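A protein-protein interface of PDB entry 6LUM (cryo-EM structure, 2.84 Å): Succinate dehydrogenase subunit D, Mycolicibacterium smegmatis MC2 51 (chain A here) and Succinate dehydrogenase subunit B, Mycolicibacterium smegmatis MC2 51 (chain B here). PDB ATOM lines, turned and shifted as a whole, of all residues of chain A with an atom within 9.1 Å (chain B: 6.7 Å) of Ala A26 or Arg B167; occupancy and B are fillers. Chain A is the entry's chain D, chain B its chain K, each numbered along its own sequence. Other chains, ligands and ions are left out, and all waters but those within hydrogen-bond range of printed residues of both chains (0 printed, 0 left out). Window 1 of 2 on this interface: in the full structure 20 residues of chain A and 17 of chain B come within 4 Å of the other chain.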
ATOM      1  N   PRO A  16      -4.272 -19.803  12.238  1.00  0.00           N
ATOM      2  CA  PRO A  16      -4.681 -18.967  11.108  1.00  0.00           C
ATOM      3  C   PRO A  16      -3.483 -18.423  10.349  1.00  0.00           C
ATOM      4  O   PRO A  16      -2.499 -17.973  10.937  1.00  0.00           O
ATOM      5  CB  PRO A  16      -5.465 -17.837  11.782  1.00  0.00           C
ATOM      6  CG  PRO A  16      -4.869 -17.742  13.136  1.00  0.00           C
ATOM      7  CD  PRO A  16      -4.517 -19.141  13.530  1.00  0.00           C
ATOM      8  N   VAL A  17      -3.579 -18.463   9.025  1.00  0.00           N
ATOM      9  CA  VAL A  17      -2.536 -17.912   8.167  1.00  0.00           C
ATOM     10  C   VAL A  17      -2.663 -16.396   8.150  1.00  0.00           C
ATOM     11  O   VAL A  17      -3.754 -15.855   7.940  1.00  0.00           O
ATOM     12  CB  VAL A  17      -2.638 -18.492   6.749  1.00  0.00           C
ATOM     13  CG1 VAL A  17      -1.415 -18.118   5.942  1.00  0.00           C
ATOM     14  CG2 VAL A  17      -2.801 -19.993   6.807  1.00  0.00           C
ATOM     15  N   MET A  18      -1.549 -15.707   8.376  1.00  0.00           N
ATOM     16  CA  MET A  18      -1.539 -14.251   8.407  1.00  0.00           C
ATOM     17  C   MET A  18      -1.131 -13.626   7.084  1.00  0.00           C
ATOM     18  O   MET A  18      -1.209 -12.401   6.947  1.00  0.00           O
ATOM     19  CB  MET A  18      -0.599 -13.753   9.506  1.00  0.00           C
ATOM     20  CG  MET A  18      -1.084 -14.037  10.909  1.00  0.00           C
ATOM     21  SD  MET A  18       0.108 -13.522  12.154  1.00  0.00           S
ATOM     22  CE  MET A  18       0.003 -11.742  12.015  1.00  0.00           C
ATOM     23  N   GLU A  19      -0.708 -14.427   6.113  1.00  0.00           N
ATOM     24  CA  GLU A  19      -0.192 -13.923   4.845  1.00  0.00           C
ATOM     25  C   GLU A  19      -1.356 -13.584   3.923  1.00  0.00           C
ATOM     26  O   GLU A  19      -2.070 -14.477   3.456  1.00  0.00           O
ATOM     27  CB  GLU A  19       0.733 -14.961   4.219  1.00  0.00           C
ATOM     28  CG  GLU A  19       1.268 -14.603   2.851  1.00  0.00           C
ATOM     29  CD  GLU A  19       1.966 -15.773   2.187  1.00  0.00           C
ATOM     30  OE1 GLU A  19       2.376 -15.640   1.018  1.00  0.00           O
ATOM     31  OE2 GLU A  19       2.103 -16.827   2.838  1.00  0.00           O
ATOM     32  N   ARG A  20      -1.551 -12.289   3.661  1.00  0.00           N
ATOM     33  CA  ARG A  20      -2.599 -11.857   2.740  1.00  0.00           C
ATOM     34  C   ARG A  20      -2.259 -12.251   1.311  1.00  0.00           C
ATOM     35  O   ARG A  20      -2.963 -13.049   0.683  1.00  0.00           O
ATOM     36  CB  ARG A  20      -2.790 -10.344   2.846  1.00  0.00           C
ATOM     37  CG  ARG A  20      -3.226  -9.875   4.215  1.00  0.00           C
ATOM     38  CD  ARG A  20      -4.631 -10.347   4.505  1.00  0.00           C
ATOM     39  NE  ARG A  20      -5.602  -9.678   3.649  1.00  0.00           N
ATOM     40  CZ  ARG A  20      -6.816 -10.150   3.384  1.00  0.00           C
ATOM     41  NH1 ARG A  20      -7.202 -11.311   3.895  1.00  0.00           N
ATOM     42  NH2 ARG A  20      -7.637  -9.467   2.597  1.00  0.00           N
ATOM     43  N   GLU A  21      -1.170 -11.704   0.786  1.00  0.00           N
ATOM     44  CA  GLU A  21      -0.647 -12.048  -0.523  1.00  0.00           C
ATOM     45  C   GLU A  21       0.862 -12.170  -0.418  1.00  0.00           C
ATOM     46  O   GLU A  21       1.456 -11.870   0.618  1.00  0.00           O
ATOM     47  CB  GLU A  21      -1.034 -11.007  -1.574  1.00  0.00           C
ATOM     48  CG  GLU A  21      -0.466  -9.631  -1.312  1.00  0.00           C
ATOM     49  CD  GLU A  21      -0.847  -8.638  -2.387  1.00  0.00           C
ATOM     50  OE1 GLU A  21      -1.570  -9.030  -3.324  1.00  0.00           O
ATOM     51  OE2 GLU A  21      -0.413  -7.471  -2.302  1.00  0.00           O
ATOM     52  N   HIS A  22       1.488 -12.607  -1.509  1.00  0.00           N
ATOM     53  CA  HIS A  22       2.915 -12.906  -1.462  1.00  0.00           C
ATOM     54  C   HIS A  22       3.742 -11.654  -1.210  1.00  0.00           C
ATOM     55  O   HIS A  22       4.751 -11.704  -0.501  1.00  0.00           O
ATOM     56  CB  HIS A  22       3.351 -13.575  -2.761  1.00  0.00           C
ATOM     57  CG  HIS A  22       4.458 -14.565  -2.583  1.00  0.00           C
ATOM     58  ND1 HIS A  22       4.301 -15.737  -1.877  1.00  0.00           N
ATOM     59  CD2 HIS A  22       5.740 -14.555  -3.016  1.00  0.00           C
ATOM     60  CE1 HIS A  22       5.437 -16.408  -1.884  1.00  0.00           C
ATOM     61  NE2 HIS A  22       6.326 -15.712  -2.570  1.00  0.00           N
ATOM     62  N   ASP A  23       3.331 -10.527  -1.773  1.00  0.00           N
ATOM     63  CA  ASP A  23       4.096  -9.293  -1.682  1.00  0.00           C
ATOM     64  C   ASP A  23       3.849  -8.534  -0.390  1.00  0.00           C
ATOM     65  O   ASP A  23       4.450  -7.476  -0.190  1.00  0.00           O
ATOM     66  CB  ASP A  23       3.754  -8.400  -2.871  1.00  0.00           C
ATOM     67  CG  ASP A  23       4.133  -9.027  -4.185  1.00  0.00           C
ATOM     68  OD1 ASP A  23       5.127  -9.775  -4.219  1.00  0.00           O
ATOM     69  OD2 ASP A  23       3.424  -8.796  -5.183  1.00  0.00           O
ATOM     70  N   ARG A  24       2.986  -9.038   0.484  1.00  0.00           N
ATOM     71  CA  ARG A  24       2.581  -8.314   1.680  1.00  0.00           C
ATOM     72  C   ARG A  24       3.220  -8.937   2.909  1.00  0.00           C
ATOM     73  O   ARG A  24       2.905 -10.089   3.243  1.00  0.00           O
ATOM     74  CB  ARG A  24       1.058  -8.325   1.813  1.00  0.00           C
ATOM     75  CG  ARG A  24       0.513  -7.370   2.849  1.00  0.00           C
ATOM     76  CD  ARG A  24       0.232  -6.026   2.240  1.00  0.00           C
ATOM     77  NE  ARG A  24       0.341  -4.944   3.209  1.00  0.00           N
ATOM     78  CZ  ARG A  24      -0.660  -4.518   3.968  1.00  0.00           C
ATOM     79  NH1 ARG A  24      -1.848  -5.090   3.878  1.00  0.00           N
ATOM     80  NH2 ARG A  24      -0.472  -3.522   4.818  1.00  0.00           N
ATOM     81  N   PRO A  25       4.119  -8.241   3.602  1.00  0.00           N
ATOM     82  CA  PRO A  25       4.598  -8.738   4.895  1.00  0.00           C
ATOM     83  C   PRO A  25       3.457  -8.807   5.897  1.00  0.00           C
ATOM     84  O   PRO A  25       2.815  -7.801   6.201  1.00  0.00           O
ATOM     85  CB  PRO A  25       5.648  -7.701   5.303  1.00  0.00           C
ATOM     86  CG  PRO A  25       6.012  -7.009   4.060  1.00  0.00           C
ATOM     87  CD  PRO A  25       4.804  -7.005   3.203  1.00  0.00           C
ATOM     88  N   ALA A  26       3.206 -10.013   6.411  1.00  0.00           N
ATOM     89  CA  ALA A  26       2.156 -10.182   7.409  1.00  0.00           C
ATOM     90  C   ALA A  26       2.416  -9.316   8.630  1.00  0.00           C
ATOM     91  O   ALA A  26       1.484  -8.754   9.214  1.00  0.00           O
ATOM     92  CB  ALA A  26       2.049 -11.650   7.811  1.00  0.00           C
ATOM     93  N   ALA A  27       3.684  -9.169   9.010  1.00  0.00           N
ATOM     94  CA  ALA A  27       4.048  -8.336  10.145  1.00  0.00           C
ATOM     95  C   ALA A  27       3.657  -6.878   9.958  1.00  0.00           C
ATOM     96  O   ALA A  27       3.807  -6.092  10.899  1.00  0.00           O
ATOM     97  CB  ALA A  27       5.549  -8.444  10.392  1.00  0.00           C
ATOM     98  N   LEU A  28       3.177  -6.497   8.774  1.00  0.00           N
ATOM     99  CA  LEU A  28       2.681  -5.144   8.566  1.00  0.00           C
ATOM    100  C   LEU A  28       1.307  -4.945   9.183  1.00  0.00           C
ATOM    101  O   LEU A  28       0.994  -3.843   9.640  1.00  0.00           O
ATOM    102  CB  LEU A  28       2.628  -4.821   7.075  1.00  0.00           C
ATOM    103  CG  LEU A  28       3.840  -4.117   6.480  1.00  0.00           C
ATOM    104  CD1 LEU A  28       3.564  -3.711   5.054  1.00  0.00           C
ATOM    105  CD2 LEU A  28       4.198  -2.918   7.308  1.00  0.00           C
ATOM    106  N   ASP A  29       0.474  -5.985   9.201  1.00  0.00           N
ATOM    107  CA  ASP A  29      -0.826  -5.924   9.851  1.00  0.00           C
ATOM    108  C   ASP A  29      -0.840  -6.688  11.168  1.00  0.00           C
ATOM    109  O   ASP A  29      -1.854  -7.289  11.533  1.00  0.00           O
ATOM    110  CB  ASP A  29      -1.920  -6.432   8.912  1.00  0.00           C
ATOM    111  CG  ASP A  29      -1.622  -7.804   8.347  1.00  0.00           C
ATOM    112  OD1 ASP A  29      -1.702  -7.965   7.110  1.00  0.00           O
ATOM    113  OD2 ASP A  29      -1.336  -8.730   9.136  1.00  0.00           O
ATOM    114  N   HIS A  30       0.282  -6.690  11.873  1.00  0.00           N
ATOM    115  CA  HIS A  30       0.338  -7.271  13.203  1.00  0.00           C
ATOM    116  C   HIS A  30      -0.591  -6.495  14.131  1.00  0.00           C
ATOM    117  O   HIS A  30      -0.698  -5.269  14.015  1.00  0.00           O
ATOM    118  CB  HIS A  30       1.772  -7.229  13.729  1.00  0.00           C
ATOM    119  CG  HIS A  30       2.046  -8.188  14.841  1.00  0.00           C
ATOM    120  ND1 HIS A  30       2.117  -9.549  14.651  1.00  0.00           N
ATOM    121  CD2 HIS A  30       2.282  -7.980  16.156  1.00  0.00           C
ATOM    122  CE1 HIS A  30       2.376 -10.140  15.802  1.00  0.00           C
ATOM    123  NE2 HIS A  30       2.485  -9.209  16.732  1.00  0.00           N
ATOM    124  N   PRO A  31      -1.285  -7.170  15.050  1.00  0.00           N
ATOM    125  CA  PRO A  31      -2.196  -6.444  15.948  1.00  0.00           C
ATOM    126  C   PRO A  31      -1.504  -5.397  16.797  1.00  0.00           C
ATOM    127  O   PRO A  31      -2.005  -4.275  16.917  1.00  0.00           O
ATOM    128  CB  PRO A  31      -2.795  -7.565  16.806  1.00  0.00           C
ATOM    129  CG  PRO A  31      -2.656  -8.786  15.979  1.00  0.00           C
ATOM    130  CD  PRO A  31      -1.366  -8.625  15.249  1.00  0.00           C
ATOM    131  N   ARG A  32      -0.358  -5.730  17.383  1.00  0.00           N
ATOM    132  CA  ARG A  32       0.354  -4.838  18.285  1.00  0.00           C
ATOM    133  C   ARG A  32       1.385  -3.974  17.576  1.00  0.00           C
ATOM    134  O   ARG A  32       2.171  -3.299  18.245  1.00  0.00           O
ATOM    135  CB  ARG A  32       1.032  -5.645  19.390  1.00  0.00           C
ATOM    136  CG  ARG A  32       0.074  -6.437  20.254  1.00  0.00           C
ATOM    137  CD  ARG A  32       0.766  -6.967  21.496  1.00  0.00           C
ATOM    138  NE  ARG A  32       1.500  -5.919  22.200  1.00  0.00           N
ATOM    139  CZ  ARG A  32       0.963  -5.094  23.092  1.00  0.00           C
ATOM    140  NH1 ARG A  32      -0.322  -5.189  23.398  1.00  0.00           N
ATOM    141  NH2 ARG A  32       1.714  -4.175  23.683  1.00  0.00           N
ATOM    142  N   ALA A  33       1.393  -3.968  16.258  1.00  0.00           N
ATOM    143  CA  ALA A  33       2.386  -3.201  15.522  1.00  0.00           C
ATOM    144  C   ALA A  33       2.001  -1.724  15.493  1.00  0.00           C
ATOM    145  O   ALA A  33       0.823  -1.392  15.353  1.00  0.00           O
ATOM    146  CB  ALA A  33       2.521  -3.726  14.100  1.00  0.00           C
ATOM    147  N   PRO B 162       2.746 -23.322   9.544  1.00  0.00           N
ATOM    148  CA  PRO B 162       3.739 -23.886   8.626  1.00  0.00           C
ATOM    149  C   PRO B 162       3.712 -23.257   7.248  1.00  0.00           C
ATOM    150  O   PRO B 162       4.557 -23.597   6.415  1.00  0.00           O
ATOM    151  CB  PRO B 162       3.354 -25.367   8.565  1.00  0.00           C
ATOM    152  CG  PRO B 162       1.953 -25.408   8.986  1.00  0.00           C
ATOM    153  CD  PRO B 162       1.793 -24.339  10.001  1.00  0.00           C
ATOM    154  N   THR B 163       2.762 -22.366   6.983  1.00  0.00           N
ATOM    155  CA  THR B 163       2.718 -21.584   5.757  1.00  0.00           C
ATOM    156  C   THR B 163       3.423 -20.249   5.896  1.00  0.00           C
ATOM    157  O   THR B 163       4.134 -19.835   4.979  1.00  0.00           O
ATOM    158  CB  THR B 163       1.266 -21.331   5.345  1.00  0.00           C
ATOM    159  OG1 THR B 163       0.588 -22.582   5.199  1.00  0.00           O
ATOM    160  CG2 THR B 163       1.213 -20.587   4.033  1.00  0.00           C
ATOM    161  N   ASP B 164       3.236 -19.574   7.029  1.00  0.00           N
ATOM    162  CA  ASP B 164       3.981 -18.357   7.311  1.00  0.00           C
ATOM    163  C   ASP B 164       5.431 -18.658   7.632  1.00  0.00           C
ATOM    164  O   ASP B 164       6.283 -17.772   7.522  1.00  0.00           O
ATOM    165  CB  ASP B 164       3.354 -17.616   8.483  1.00  0.00           C
ATOM    166  CG  ASP B 164       1.872 -17.428   8.327  1.00  0.00           C
ATOM    167  OD1 ASP B 164       1.438 -16.981   7.249  1.00  0.00           O
ATOM    168  OD2 ASP B 164       1.138 -17.730   9.285  1.00  0.00           O
ATOM    169  N   ARG B 165       5.726 -19.883   8.059  1.00  0.00           N
ATOM    170  CA  ARG B 165       7.100 -20.240   8.373  1.00  0.00           C
ATOM    171  C   ARG B 165       7.915 -20.444   7.106  1.00  0.00           C
ATOM    172  O   ARG B 165       9.068 -20.014   7.029  1.00  0.00           O
ATOM    173  CB  ARG B 165       7.123 -21.491   9.248  1.00  0.00           C
ATOM    174  CG  ARG B 165       8.400 -22.295   9.169  1.00  0.00           C
ATOM    175  CD  ARG B 165       9.504 -21.661   9.976  1.00  0.00           C
ATOM    176  NE  ARG B 165      10.756 -22.394   9.839  1.00  0.00           N
ATOM    177  CZ  ARG B 165      11.822 -21.939   9.195  1.00  0.00           C
ATOM    178  NH1 ARG B 165      11.788 -20.749   8.624  1.00  0.00           N
ATOM    179  NH2 ARG B 165      12.921 -22.672   9.121  1.00  0.00           N
ATOM    180  N   ALA B 166       7.331 -21.072   6.096  1.00  0.00           N
ATOM    181  CA  ALA B 166       8.045 -21.381   4.868  1.00  0.00           C
ATOM    182  C   ALA B 166       8.204 -20.181   3.955  1.00  0.00           C
ATOM    183  O   ALA B 166       8.591 -20.351   2.797  1.00  0.00           O
ATOM    184  CB  ALA B 166       7.333 -22.502   4.117  1.00  0.00           C
ATOM    185  N   ARG B 167       7.921 -18.980   4.439  1.00  0.00           N
ATOM    186  CA  ARG B 167       8.033 -17.784   3.620  1.00  0.00           C
ATOM    187  C   ARG B 167       9.396 -17.126   3.767  1.00  0.00           C
ATOM    188  O   ARG B 167      10.050 -16.826   2.767  1.00  0.00           O
ATOM    189  CB  ARG B 167       6.929 -16.798   3.988  1.00  0.00           C
ATOM    190  CG  ARG B 167       6.593 -15.808   2.913  1.00  0.00           C
ATOM    191  CD  ARG B 167       6.091 -14.546   3.554  1.00  0.00           C
ATOM    192  NE  ARG B 167       5.170 -13.790   2.714  1.00  0.00           N
ATOM    193  CZ  ARG B 167       4.510 -12.716   3.132  1.00  0.00           C
ATOM    194  NH1 ARG B 167       4.670 -12.282   4.374  1.00  0.00           N
ATOM    195  NH2 ARG B 167       3.688 -12.080   2.316  1.00  0.00           N
ATOM    196  N   TYR B 168       9.839 -16.894   4.995  1.00  0.00           N
ATOM    197  CA  TYR B 168      11.159 -16.337   5.234  1.00  0.00           C
ATOM    198  C   TYR B 168      12.235 -17.397   5.273  1.00  0.00           C
ATOM    199  O   TYR B 168      13.356 -17.105   5.680  1.00  0.00           O
ATOM    200  CB  TYR B 168      11.181 -15.535   6.531  1.00  0.00           C
ATOM    201  CG  TYR B 168      10.854 -16.313   7.776  1.00  0.00           C
ATOM    202  CD1 TYR B 168       9.557 -16.421   8.224  1.00  0.00           C
ATOM    203  CD2 TYR B 168      11.849 -16.912   8.520  1.00  0.00           C
ATOM    204  CE1 TYR B 168       9.262 -17.110   9.355  1.00  0.00           C
ATOM    205  CE2 TYR B 168      11.558 -17.603   9.651  1.00  0.00           C
ATOM    206  CZ  TYR B 168      10.264 -17.698  10.069  1.00  0.00           C
ATOM    207  OH  TYR B 168       9.963 -18.394  11.212  1.00  0.00           O
ATOM    208  N   ASP B 169      11.921 -18.618   4.872  1.00  0.00           N
ATOM    209  CA  ASP B 169      12.942 -19.613   4.641  1.00  0.00           C
ATOM    210  C   ASP B 169      13.868 -19.145   3.522  1.00  0.00           C
ATOM    211  O   ASP B 169      13.594 -18.173   2.818  1.00  0.00           O
ATOM    212  CB  ASP B 169      12.292 -20.941   4.282  1.00  0.00           C
ATOM    213  CG  ASP B 169      13.250 -22.086   4.318  1.00  0.00           C
ATOM    214  OD1 ASP B 169      13.137 -22.927   5.229  1.00  0.00           O
ATOM    215  OD2 ASP B 169      14.117 -22.152   3.426  1.00  0.00           O
ATOM    216  N   ASP B 170      14.997 -19.833   3.388  1.00  0.00           N
ATOM    217  CA  ASP B 170      15.974 -19.597   2.329  1.00  0.00           C
ATOM    218  C   ASP B 170      16.764 -18.316   2.556  1.00  0.00           C
ATOM    219  O   ASP B 170      17.778 -18.091   1.902  1.00  0.00           O
ATOM    220  CB  ASP B 170      15.287 -19.580   0.960  1.00  0.00           C
ATOM    221  CG  ASP B 170      16.202 -19.133  -0.153  1.00  0.00           C
ATOM    222  OD1 ASP B 170      16.969 -19.962  -0.679  1.00  0.00           O
ATOM    223  OD2 ASP B 170      16.146 -17.944  -0.505  1.00  0.00           O
ATOM    224  N   THR B 171      16.360 -17.502   3.518  1.00  0.00           N
ATOM    225  CA  THR B 171      17.198 -16.422   4.000  1.00  0.00           C
ATOM    226  C   THR B 171      17.659 -16.674   5.417  1.00  0.00           C
ATOM    227  O   THR B 171      18.384 -15.853   5.979  1.00  0.00           O
ATOM    228  CB  THR B 171      16.470 -15.084   3.926  1.00  0.00           C
ATOM    229  OG1 THR B 171      15.125 -15.253   4.364  1.00  0.00           O
ATOM    230  CG2 THR B 171      16.466 -14.570   2.520  1.00  0.00           C
ATOM    231  N   HIS B 203      15.362  -9.081   5.099  1.00  0.00           N
ATOM    232  CA  HIS B 203      14.266  -9.838   4.510  1.00  0.00           C
ATOM    233  C   HIS B 203      13.792 -10.919   5.459  1.00  0.00           C
ATOM    234  O   HIS B 203      12.584 -11.135   5.623  1.00  0.00           O
ATOM    235  CB  HIS B 203      14.741 -10.433   3.186  1.00  0.00           C
ATOM    236  CG  HIS B 203      13.788 -11.394   2.550  1.00  0.00           C
ATOM    237  ND1 HIS B 203      13.702 -12.713   2.923  1.00  0.00           N
ATOM    238  CD2 HIS B 203      12.932 -11.243   1.515  1.00  0.00           C
ATOM    239  CE1 HIS B 203      12.809 -13.326   2.170  1.00  0.00           C
ATOM    240  NE2 HIS B 203      12.329 -12.455   1.307  1.00  0.00           N
ATOM    241  N   ILE B 206      11.617  -9.057   7.978  1.00  0.00           N
ATOM    242  CA  ILE B 206      10.469  -8.363   7.421  1.00  0.00           C
ATOM    243  C   ILE B 206       9.387  -9.360   7.052  1.00  0.00           C
ATOM    244  O   ILE B 206       8.196  -9.095   7.236  1.00  0.00           O
ATOM    245  CB  ILE B 206      10.907  -7.512   6.219  1.00  0.00           C
ATOM    246  CG1 ILE B 206      11.600  -6.247   6.702  1.00  0.00           C
ATOM    247  CG2 ILE B 206       9.738  -7.166   5.360  1.00  0.00           C
ATOM    248  CD1 ILE B 206      12.423  -5.591   5.660  1.00  0.00           C
ATOM    249  N   PHE B 207       9.772 -10.532   6.558  1.00  0.00           N
ATOM    250  CA  PHE B 207       8.782 -11.524   6.169  1.00  0.00           C
ATOM    251  C   PHE B 207       8.566 -12.580   7.241  1.00  0.00           C
ATOM    252  O   PHE B 207       8.224 -13.721   6.932  1.00  0.00           O
ATOM    253  CB  PHE B 207       9.171 -12.146   4.836  1.00  0.00           C
ATOM    254  CG  PHE B 207       8.987 -11.212   3.685  1.00  0.00           C
ATOM    255  CD1 PHE B 207       9.903 -10.216   3.430  1.00  0.00           C
ATOM    256  CD2 PHE B 207       7.876 -11.291   2.889  1.00  0.00           C
ATOM    257  CE1 PHE B 207       9.725  -9.351   2.396  1.00  0.00           C
ATOM    258  CE2 PHE B 207       7.703 -10.423   1.854  1.00  0.00           C
ATOM    259  CZ  PHE B 207       8.627  -9.457   1.610  1.00  0.00           C
ATOM    260  N   ASP B 208       8.733 -12.201   8.503  1.00  0.00           N
ATOM    261  CA  ASP B 208       8.464 -13.050   9.657  1.00  0.00           C
ATOM    262  C   ASP B 208       7.171 -12.586  10.308  1.00  0.00           C
ATOM    263  O   ASP B 208       7.046 -11.414  10.670  1.00  0.00           O
ATOM    264  CB  ASP B 208       9.615 -12.984  10.656  1.00  0.00           C
ATOM    265  CG  ASP B 208       9.574 -14.098  11.661  1.00  0.00           C
ATOM    266  OD1 ASP B 208       8.752 -15.011  11.494  1.00  0.00           O
ATOM    267  OD2 ASP B 208      10.367 -14.071  12.619  1.00  0.00           O
ATOM    268  N   SER B 209       6.217 -13.504  10.463  1.00  0.00           N
ATOM    269  CA  SER B 209       4.902 -13.130  10.969  1.00  0.00           C
ATOM    270  C   SER B 209       4.976 -12.566  12.377  1.00  0.00           C
ATOM    271  O   SER B 209       4.306 -11.577  12.691  1.00  0.00           O
ATOM    272  CB  SER B 209       3.973 -14.333  10.939  1.00  0.00           C
ATOM    273  OG  SER B 209       4.037 -14.959   9.683  1.00  0.00           O
ATOM    274  N   ASP B 211       6.666 -10.568  14.107  1.00  0.00           N
ATOM    275  CA  ASP B 211       7.530  -9.409  14.238  1.00  0.00           C
ATOM    276  C   ASP B 211       6.684  -8.145  14.213  1.00  0.00           C
ATOM    277  O   ASP B 211       5.660  -8.078  13.533  1.00  0.00           O
ATOM    278  CB  ASP B 211       8.577  -9.372  13.121  1.00  0.00           C
ATOM    279  CG  ASP B 211       9.751  -8.486  13.455  1.00  0.00           C
ATOM    280  OD1 ASP B 211      10.008  -8.261  14.648  1.00  0.00           O
ATOM    281  OD2 ASP B 211      10.417  -8.006  12.522  1.00  0.00           O
ATOM    282  N   ALA B 214       8.372  -4.684  11.115  1.00  0.00           N
ATOM    283  CA  ALA B 214       8.512  -4.809   9.672  1.00  0.00           C
ATOM    284  C   ALA B 214       8.466  -3.451   9.000  1.00  0.00           C
ATOM    285  O   ALA B 214       9.270  -3.164   8.108  1.00  0.00           O
ATOM    286  CB  ALA B 214       7.421  -5.710   9.113  1.00  0.00           C
ATOM    287  N   GLU B 252      12.228  -9.117  -3.703  1.00  0.00           N
ATOM    288  CA  GLU B 252      11.035  -9.210  -2.874  1.00  0.00           C
ATOM    289  C   GLU B 252      10.927  -8.039  -1.919  1.00  0.00           C
ATOM    290  O   GLU B 252       9.823  -7.565  -1.650  1.00  0.00           O
ATOM    291  CB  GLU B 252      11.030 -10.516  -2.104  1.00  0.00           C
ATOM    292  CG  GLU B 252      10.965 -11.721  -2.987  1.00  0.00           C
ATOM    293  CD  GLU B 252      10.725 -12.986  -2.208  1.00  0.00           C
ATOM    294  OE1 GLU B 252      10.222 -12.892  -1.073  1.00  0.00           O
ATOM    295  OE2 GLU B 252      11.035 -14.077  -2.723  1.00  0.00           O
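The backbone NH of Met A18 sits at hydrogen-bond distance from the side-chain carboxylate of Asp B164 (3.4 Å). The backbone NH (N) of Ala A26 lies close to the guanidinium group (NH1) of Arg B167. The side-chain carboxylate (OE1) of Glu A19 is in salt-bridge range of the guanidinium group (NE) of Arg B167, 3.8 Å away. O of His A22 lies within hydrogen-bond range of NH2 of Arg B167. The guanidinium group (NH2) of Arg B167 lies within hydrogen-bond range of the backbone carbonyl oxygen (O) of Glu A21 (2.8 Å). The guanidinium group (NH1) of Arg B167 is in hydrogen-bond range of the backbone carbonyl oxygen (O) of Arg A24, at 3.0 Å.
Of the 18 printed residues of chain A, 10 touch a printed residue of chain B. Printed residues of chain A that touch a printed residue of chain B: Val A17, Met A18, Glu A19, Glu A21, His A22, Arg A24, Pro A25, Ala A26, Ala A27 and His A30. Hydrophobic or aromatic side chains of chain A within 4 Å of the printed part of chain B: Val A17, Pro A25, Ala A27 and His A30. Hydrophobic or aromatic side chains of chain B within 4 Å of the printed part of chain A: Ile B206, Phe B207 and Ala B214. Among the printed residues, 16 pairs touch across the chains. Among the printed residues, Asp or Glu carboxylates within 4 Å of a Lys or Arg side-chain nitrogen of the other chain: Glu A19 with Arg B167 (3.8 Å).
Among the printed residues, pairs that only touch across the chains: Val A17 with Asp B164 (3.3 Å), Glu A19 with Asp B164 (3.5 Å), His A22 with Phe B207 (3.99 Å), Pro A25 with Arg B167 (3.6 Å), Pro A25 with Ile B206 (3.5 Å), Ala A27 with Asp B208 (3.3 Å), Ala A27 with Asp B211 (3.2 Å), Ala A27 with Ala B214 (3.6 Å), His A30 with Ser B209 (3.6 Å) and His A30 with Asp B211 (3.8 Å).
ND1 of His A22 is in hydrogen-bond range of OE1 of Glu A19 (3.5 Å).
Ala A26 touches just one residue of chain B: Arg B167. Arg B167 touches just these residues of chain A: Glu A19, Glu A21, His A22, Arg A24, Pro A25 and Ala A26. No residue of chain A comes within 4 Å of Ala B166. Of the printed residues of chain B, Val A17 touches Asp B164 (3.3 Å). Printed residues of chain A within 4 Å of Phe B207: His A22. Of the printed residues of chain A, Ile B206 touches Pro A25 (3.5 Å). Printed residues of chain B within 4 Å of Glu A19: Asp B164 and Arg B167.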
